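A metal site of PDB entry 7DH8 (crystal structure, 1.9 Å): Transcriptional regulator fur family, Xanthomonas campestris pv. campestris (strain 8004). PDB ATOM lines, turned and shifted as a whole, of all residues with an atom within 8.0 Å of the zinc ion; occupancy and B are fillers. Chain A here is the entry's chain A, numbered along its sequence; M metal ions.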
ATOM      1  N   GLY A  94     -14.867   3.060   1.413  1.00  0.00           N
ATOM      2  CA  GLY A  94     -16.205   2.762   1.896  1.00  0.00           C
ATOM      3  C   GLY A  94     -16.314   1.686   2.948  1.00  0.00           C
ATOM      4  O   GLY A  94     -17.415   1.172   3.152  1.00  0.00           O
ATOM      5  N   PHE A  95     -15.220   1.332   3.627  1.00  0.00           N
ATOM      6  CA  PHE A  95     -15.306   0.384   4.733  1.00  0.00           C
ATOM      7  C   PHE A  95     -15.666   1.036   6.073  1.00  0.00           C
ATOM      8  O   PHE A  95     -16.043   0.334   6.997  1.00  0.00           O
ATOM      9  CB  PHE A  95     -13.977  -0.382   4.877  1.00  0.00           C
ATOM     10  CG  PHE A  95     -13.552  -1.072   3.614  1.00  0.00           C
ATOM     11  CD1 PHE A  95     -14.351  -2.082   3.048  1.00  0.00           C
ATOM     12  CD2 PHE A  95     -12.375  -0.731   2.966  1.00  0.00           C
ATOM     13  CE1 PHE A  95     -13.983  -2.728   1.888  1.00  0.00           C
ATOM     14  CE2 PHE A  95     -11.993  -1.381   1.809  1.00  0.00           C
ATOM     15  CZ  PHE A  95     -12.796  -2.372   1.255  1.00  0.00           C
ATOM     16  N   VAL A  96     -15.533   2.353   6.178  1.00  0.00           N
ATOM     17  CA  VAL A  96     -15.796   3.089   7.410  1.00  0.00           C
ATOM     18  C   VAL A  96     -16.521   4.340   6.983  1.00  0.00           C
ATOM     19  O   VAL A  96     -16.210   4.904   5.927  1.00  0.00           O
ATOM     20  CB  VAL A  96     -14.493   3.428   8.159  1.00  0.00           C
ATOM     21  CG1 VAL A  96     -14.668   4.702   9.058  1.00  0.00           C
ATOM     22  CG2 VAL A  96     -13.966   2.199   8.945  1.00  0.00           C
ATOM     23  N   HIS A  97     -17.528   4.755   7.734  1.00  0.00           N
ATOM     24  CA  HIS A  97     -18.229   5.983   7.431  1.00  0.00           C
ATOM     25  C   HIS A  97     -17.904   6.986   8.512  1.00  0.00           C
ATOM     26  O   HIS A  97     -17.899   6.639   9.690  1.00  0.00           O
ATOM     27  CB  HIS A  97     -19.756   5.791   7.375  1.00  0.00           C
ATOM     28  CG  HIS A  97     -20.207   4.847   6.302  1.00  0.00           C
ATOM     29  ND1 HIS A  97     -20.345   5.245   4.990  1.00  0.00           N
ATOM     30  CD2 HIS A  97     -20.571   3.545   6.339  1.00  0.00           C
ATOM     31  CE1 HIS A  97     -20.746   4.216   4.255  1.00  0.00           C
ATOM     32  NE2 HIS A  97     -20.927   3.182   5.060  1.00  0.00           N
ATOM     33  N   VAL A 106     -17.845   4.828  12.045  1.00  0.00           N
ATOM     34  CA  VAL A 106     -18.559   3.573  12.239  1.00  0.00           C
ATOM     35  C   VAL A 106     -18.134   2.674  11.082  1.00  0.00           C
ATOM     36  O   VAL A 106     -17.808   3.170   9.994  1.00  0.00           O
ATOM     37  CB  VAL A 106     -20.135   3.689  12.280  1.00  0.00           C
ATOM     38  CG1 VAL A 106     -20.670   4.283  13.570  1.00  0.00           C
ATOM     39  CG2 VAL A 106     -20.702   4.479  11.025  1.00  0.00           C
ATOM     40  N   ALA A 107     -18.111   1.369  11.313  1.00  0.00           N
ATOM     41  CA  ALA A 107     -17.759   0.454  10.246  1.00  0.00           C
ATOM     42  C   ALA A 107     -18.957   0.305   9.314  1.00  0.00           C
ATOM     43  O   ALA A 107     -20.123   0.346   9.754  1.00  0.00           O
ATOM     44  CB  ALA A 107     -17.319  -0.898  10.796  1.00  0.00           C
ATOM     45  N   CYS A 108     -18.674   0.160   8.024  1.00  0.00           N
ATOM     46  CA  CYS A 108     -19.782  -0.121   7.121  1.00  0.00           C
ATOM     47  C   CYS A 108     -20.237  -1.577   7.282  1.00  0.00           C
ATOM     48  O   CYS A 108     -19.432  -2.513   7.201  1.00  0.00           O
ATOM     49  CB  CYS A 108     -19.404   0.147   5.670  1.00  0.00           C
ATOM     50  SG  CYS A 108     -20.792  -0.310   4.466  1.00  0.00           S
ATOM     51  N   HIS A 109     -21.531  -1.747   7.523  1.00  0.00           N
ATOM     52  CA  HIS A 109     -22.165  -3.030   7.768  1.00  0.00           C
ATOM     53  C   HIS A 109     -22.100  -3.954   6.524  1.00  0.00           C
ATOM     54  O   HIS A 109     -22.006  -5.180   6.699  1.00  0.00           O
ATOM     55  CB  HIS A 109     -23.503  -2.805   8.490  1.00  0.00           C
ATOM     56  CG  HIS A 109     -24.593  -2.290   7.605  1.00  0.00           C
ATOM     57  ND1 HIS A 109     -25.909  -2.707   7.703  1.00  0.00           N
ATOM     58  CD2 HIS A 109     -24.569  -1.408   6.569  1.00  0.00           C
ATOM     59  CE1 HIS A 109     -26.646  -2.107   6.789  1.00  0.00           C
ATOM     60  NE2 HIS A 109     -25.858  -1.313   6.076  1.00  0.00           N
ATOM     61  N   HIS A 110     -22.140  -3.392   5.283  1.00  0.00           N
ATOM     62  CA  HIS A 110     -21.937  -4.139   4.032  1.00  0.00           C
ATOM     63  C   HIS A 110     -20.894  -3.416   3.197  1.00  0.00           C
ATOM     64  O   HIS A 110     -21.164  -2.358   2.611  1.00  0.00           O
ATOM     65  CB  HIS A 110     -23.314  -4.170   3.395  1.00  0.00           C
ATOM     66  CG  HIS A 110     -24.194  -5.234   3.984  1.00  0.00           C
ATOM     67  ND1 HIS A 110     -23.826  -6.562   3.995  1.00  0.00           N
ATOM     68  CD2 HIS A 110     -25.357  -5.142   4.675  1.00  0.00           C
ATOM     69  CE1 HIS A 110     -24.745  -7.263   4.633  1.00  0.00           C
ATOM     70  NE2 HIS A 110     -25.688  -6.430   5.067  1.00  0.00           N
ATOM     71  N   PRO A 111     -19.701  -4.012   3.085  1.00  0.00           N
ATOM     72  CA  PRO A 111     -18.504  -3.227   2.770  1.00  0.00           C
ATOM     73  C   PRO A 111     -18.290  -3.129   1.267  1.00  0.00           C
ATOM     74  O   PRO A 111     -17.792  -2.101   0.787  1.00  0.00           O
ATOM     75  CB  PRO A 111     -17.298  -3.959   3.379  1.00  0.00           C
ATOM     76  CG  PRO A 111     -17.781  -5.377   3.556  1.00  0.00           C
ATOM     77  CD  PRO A 111     -19.216  -5.224   3.972  1.00  0.00           C
ATOM     78  N   ASN A 112     -18.648  -4.180   0.507  1.00  0.00           N
ATOM     79  CA  ASN A 112     -18.330  -4.100  -0.927  1.00  0.00           C
ATOM     80  C   ASN A 112     -19.673  -3.448  -1.323  1.00  0.00           C
ATOM     81  O   ASN A 112     -20.519  -4.111  -1.907  1.00  0.00           O
ATOM     82  CB  ASN A 112     -18.171  -5.481  -1.583  1.00  0.00           C
ATOM     83  CG  ASN A 112     -19.453  -6.317  -1.513  1.00  0.00           C
ATOM     84  OD1 ASN A 112     -20.421  -5.962  -0.831  1.00  0.00           O
ATOM     85  ND2 ASN A 112     -19.439  -7.459  -2.204  1.00  0.00           N
ATOM     86  N   SER A 113     -19.952  -2.165  -1.107  1.00  0.00           N
ATOM     87  CA  SER A 113     -21.109  -1.530  -1.743  1.00  0.00           C
ATOM     88  C   SER A 113     -20.272  -0.413  -2.375  1.00  0.00           C
ATOM     89  O   SER A 113     -20.809   0.648  -2.711  1.00  0.00           O
ATOM     90  CB  SER A 113     -22.231  -0.991  -0.839  1.00  0.00           C
ATOM     91  OG  SER A 113     -21.838  -0.851   0.523  1.00  0.00           O
ATOM     92  N   ALA A 114     -18.970  -0.664  -2.590  1.00  0.00           N
ATOM     93  CA  ALA A 114     -17.988   0.338  -3.013  1.00  0.00           C
ATOM     94  C   ALA A 114     -18.039   1.497  -2.033  1.00  0.00           C
ATOM     95  O   ALA A 114     -18.064   1.271  -0.815  1.00  0.00           O
ATOM     96  CB  ALA A 114     -18.207   0.836  -4.453  1.00  0.00           C
ATOM     97  N   GLN A 115     -18.031   2.736  -2.514  1.00  0.00           N
ATOM     98  CA  GLN A 115     -18.378   3.861  -1.667  1.00  0.00           C
ATOM     99  C   GLN A 115     -19.762   4.310  -2.101  1.00  0.00           C
ATOM    100  O   GLN A 115     -20.128   4.171  -3.268  1.00  0.00           O
ATOM    101  CB  GLN A 115     -17.375   5.021  -1.750  1.00  0.00           C
ATOM    102  CG  GLN A 115     -17.474   5.927  -2.990  1.00  0.00           C
ATOM    103  CD  GLN A 115     -16.178   6.715  -3.263  1.00  0.00           C
ATOM    104  OE1 GLN A 115     -15.371   6.344  -4.127  1.00  0.00           O
ATOM    105  NE2 GLN A 115     -15.963   7.790  -2.502  1.00  0.00           N
ATOM    106  N   HIS A 116     -20.530   4.807  -1.151  1.00  0.00           N
ATOM    107  CA  HIS A 116     -21.966   4.908  -1.343  1.00  0.00           C
ATOM    108  C   HIS A 116     -22.480   5.926  -0.368  1.00  0.00           C
ATOM    109  O   HIS A 116     -21.912   6.129   0.704  1.00  0.00           O
ATOM    110  CB  HIS A 116     -22.650   3.566  -1.083  1.00  0.00           C
ATOM    111  CG  HIS A 116     -22.338   2.995   0.260  1.00  0.00           C
ATOM    112  ND1 HIS A 116     -21.107   2.467   0.572  1.00  0.00           N
ATOM    113  CD2 HIS A 116     -23.081   2.896   1.388  1.00  0.00           C
ATOM    114  CE1 HIS A 116     -21.113   2.027   1.820  1.00  0.00           C
ATOM    115  NE2 HIS A 116     -22.301   2.286   2.338  1.00  0.00           N
ATOM    116  N   SER A 117     -23.651   6.448  -0.686  1.00  0.00           N
ATOM    117  CA  SER A 117     -24.345   7.378   0.174  1.00  0.00           C
ATOM    118  C   SER A 117     -25.563   6.658   0.728  1.00  0.00           C
ATOM    119  O   SER A 117     -26.276   5.989  -0.031  1.00  0.00           O
ATOM    120  CB  SER A 117     -24.735   8.628  -0.632  1.00  0.00           C
ATOM    121  OG  SER A 117     -23.510   9.313  -0.854  1.00  0.00           O
ATOM    122  N   VAL A 118     -25.743   6.745   2.056  1.00  0.00           N
ATOM    123  CA  VAL A 118     -26.838   6.028   2.728  1.00  0.00           C
ATOM    124  C   VAL A 118     -27.297   6.804   3.950  1.00  0.00           C
ATOM    125  O   VAL A 118     -26.490   7.467   4.586  1.00  0.00           O
ATOM    126  CB  VAL A 118     -26.441   4.605   3.181  1.00  0.00           C
ATOM    127  CG1 VAL A 118     -26.244   3.685   2.007  1.00  0.00           C
ATOM    128  CG2 VAL A 118     -25.218   4.671   4.165  1.00  0.00           C
ATOM    129  N   PRO A 119     -28.562   6.723   4.311  1.00  0.00           N
ATOM    130  CA  PRO A 119     -29.020   7.309   5.574  1.00  0.00           C
ATOM    131  C   PRO A 119     -28.502   6.520   6.769  1.00  0.00           C
ATOM    132  O   PRO A 119     -28.360   5.296   6.755  1.00  0.00           O
ATOM    133  CB  PRO A 119     -30.559   7.178   5.481  1.00  0.00           C
ATOM    134  CG  PRO A 119     -30.829   6.918   3.971  1.00  0.00           C
ATOM    135  CD  PRO A 119     -29.651   6.118   3.539  1.00  0.00           C
ATOM    136  N   PHE A 120     -28.328   7.267   7.832  1.00  0.00           N
ATOM    137  CA  PHE A 120     -28.067   6.801   9.181  1.00  0.00           C
ATOM    138  C   PHE A 120     -29.119   7.341  10.115  1.00  0.00           C
ATOM    139  O   PHE A 120     -29.464   8.525  10.016  1.00  0.00           O
ATOM    140  CB  PHE A 120     -26.685   7.320   9.664  1.00  0.00           C
ATOM    141  CG  PHE A 120     -25.571   6.643   8.996  1.00  0.00           C
ATOM    142  CD1 PHE A 120     -25.075   7.151   7.814  1.00  0.00           C
ATOM    143  CD2 PHE A 120     -25.045   5.479   9.514  1.00  0.00           C
ATOM    144  CE1 PHE A 120     -24.081   6.492   7.137  1.00  0.00           C
ATOM    145  CE2 PHE A 120     -24.042   4.818   8.825  1.00  0.00           C
ATOM    146  CZ  PHE A 120     -23.564   5.330   7.666  1.00  0.00           C
ATOM    147  N   GLU A 131     -27.232   2.102  10.016  1.00  0.00           N
ATOM    148  CA  GLU A 131     -26.970   2.388   8.624  1.00  0.00           C
ATOM    149  C   GLU A 131     -28.047   1.731   7.777  1.00  0.00           C
ATOM    150  O   GLU A 131     -28.196   0.521   7.826  1.00  0.00           O
ATOM    151  CB  GLU A 131     -25.615   1.821   8.189  1.00  0.00           C
ATOM    152  CG  GLU A 131     -25.350   2.157   6.690  1.00  0.00           C
ATOM    153  CD  GLU A 131     -23.983   1.674   6.207  1.00  0.00           C
ATOM    154  OE1 GLU A 131     -23.148   1.250   7.043  1.00  0.00           O
ATOM    155  OE2 GLU A 131     -23.709   1.750   4.976  1.00  0.00           O
ATOM    156  N   LEU A 132     -28.761   2.515   6.973  1.00  0.00           N
ATOM    157  CA  LEU A 132     -29.762   1.979   6.078  1.00  0.00           C
ATOM    158  C   LEU A 132     -29.215   1.979   4.650  1.00  0.00           C
ATOM    159  O   LEU A 132     -28.069   2.383   4.380  1.00  0.00           O
ATOM    160  CB  LEU A 132     -31.058   2.812   6.170  1.00  0.00           C
ATOM    161  CG  LEU A 132     -31.636   3.021   7.586  1.00  0.00           C
ATOM    162  CD1 LEU A 132     -33.007   3.685   7.506  1.00  0.00           C
ATOM    163  CD2 LEU A 132     -31.757   1.669   8.304  1.00  0.00           C
HETATM  164 ZN    ZN M   1     -21.787   1.494   4.376  1.00  0.00          ZN
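The backbone carbonyl oxygen of Val 106 is in hydrogen-bond range of the backbone NH of His 97 (2.8 Å).
OE1 of Glu 131 sits close to N of His 109, at 3.4 Å.
The side-chain sulfur (SG) of Cys 108 lies close to the backbone carbonyl oxygen (O) of His 110 (2.8 Å).
O of Phe 95 lies within hydrogen-bond range of N of Cys 108 (2.8 Å).
ND1 of His 116 sits close to OG of Ser 113.
Four residues have an atom within 4 Å of the zinc ion: His 97, Cys 108, His 116 and Glu 131.
The nearest printed residue that does not touch the zinc ion is His 110 (4.3 Å).
A ring nitrogen (NE2) of His 97 is bound to the zinc ion, 2.0 Å away.
The zinc ion is bound by OE2 of Glu 131.
The zinc ion is bound by SG of Cys 108, 2.1 Å away.
The zinc ion is bound by NE2 of His 116 (2.2 Å).
The zinc ion has four donor atoms within binding distance.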
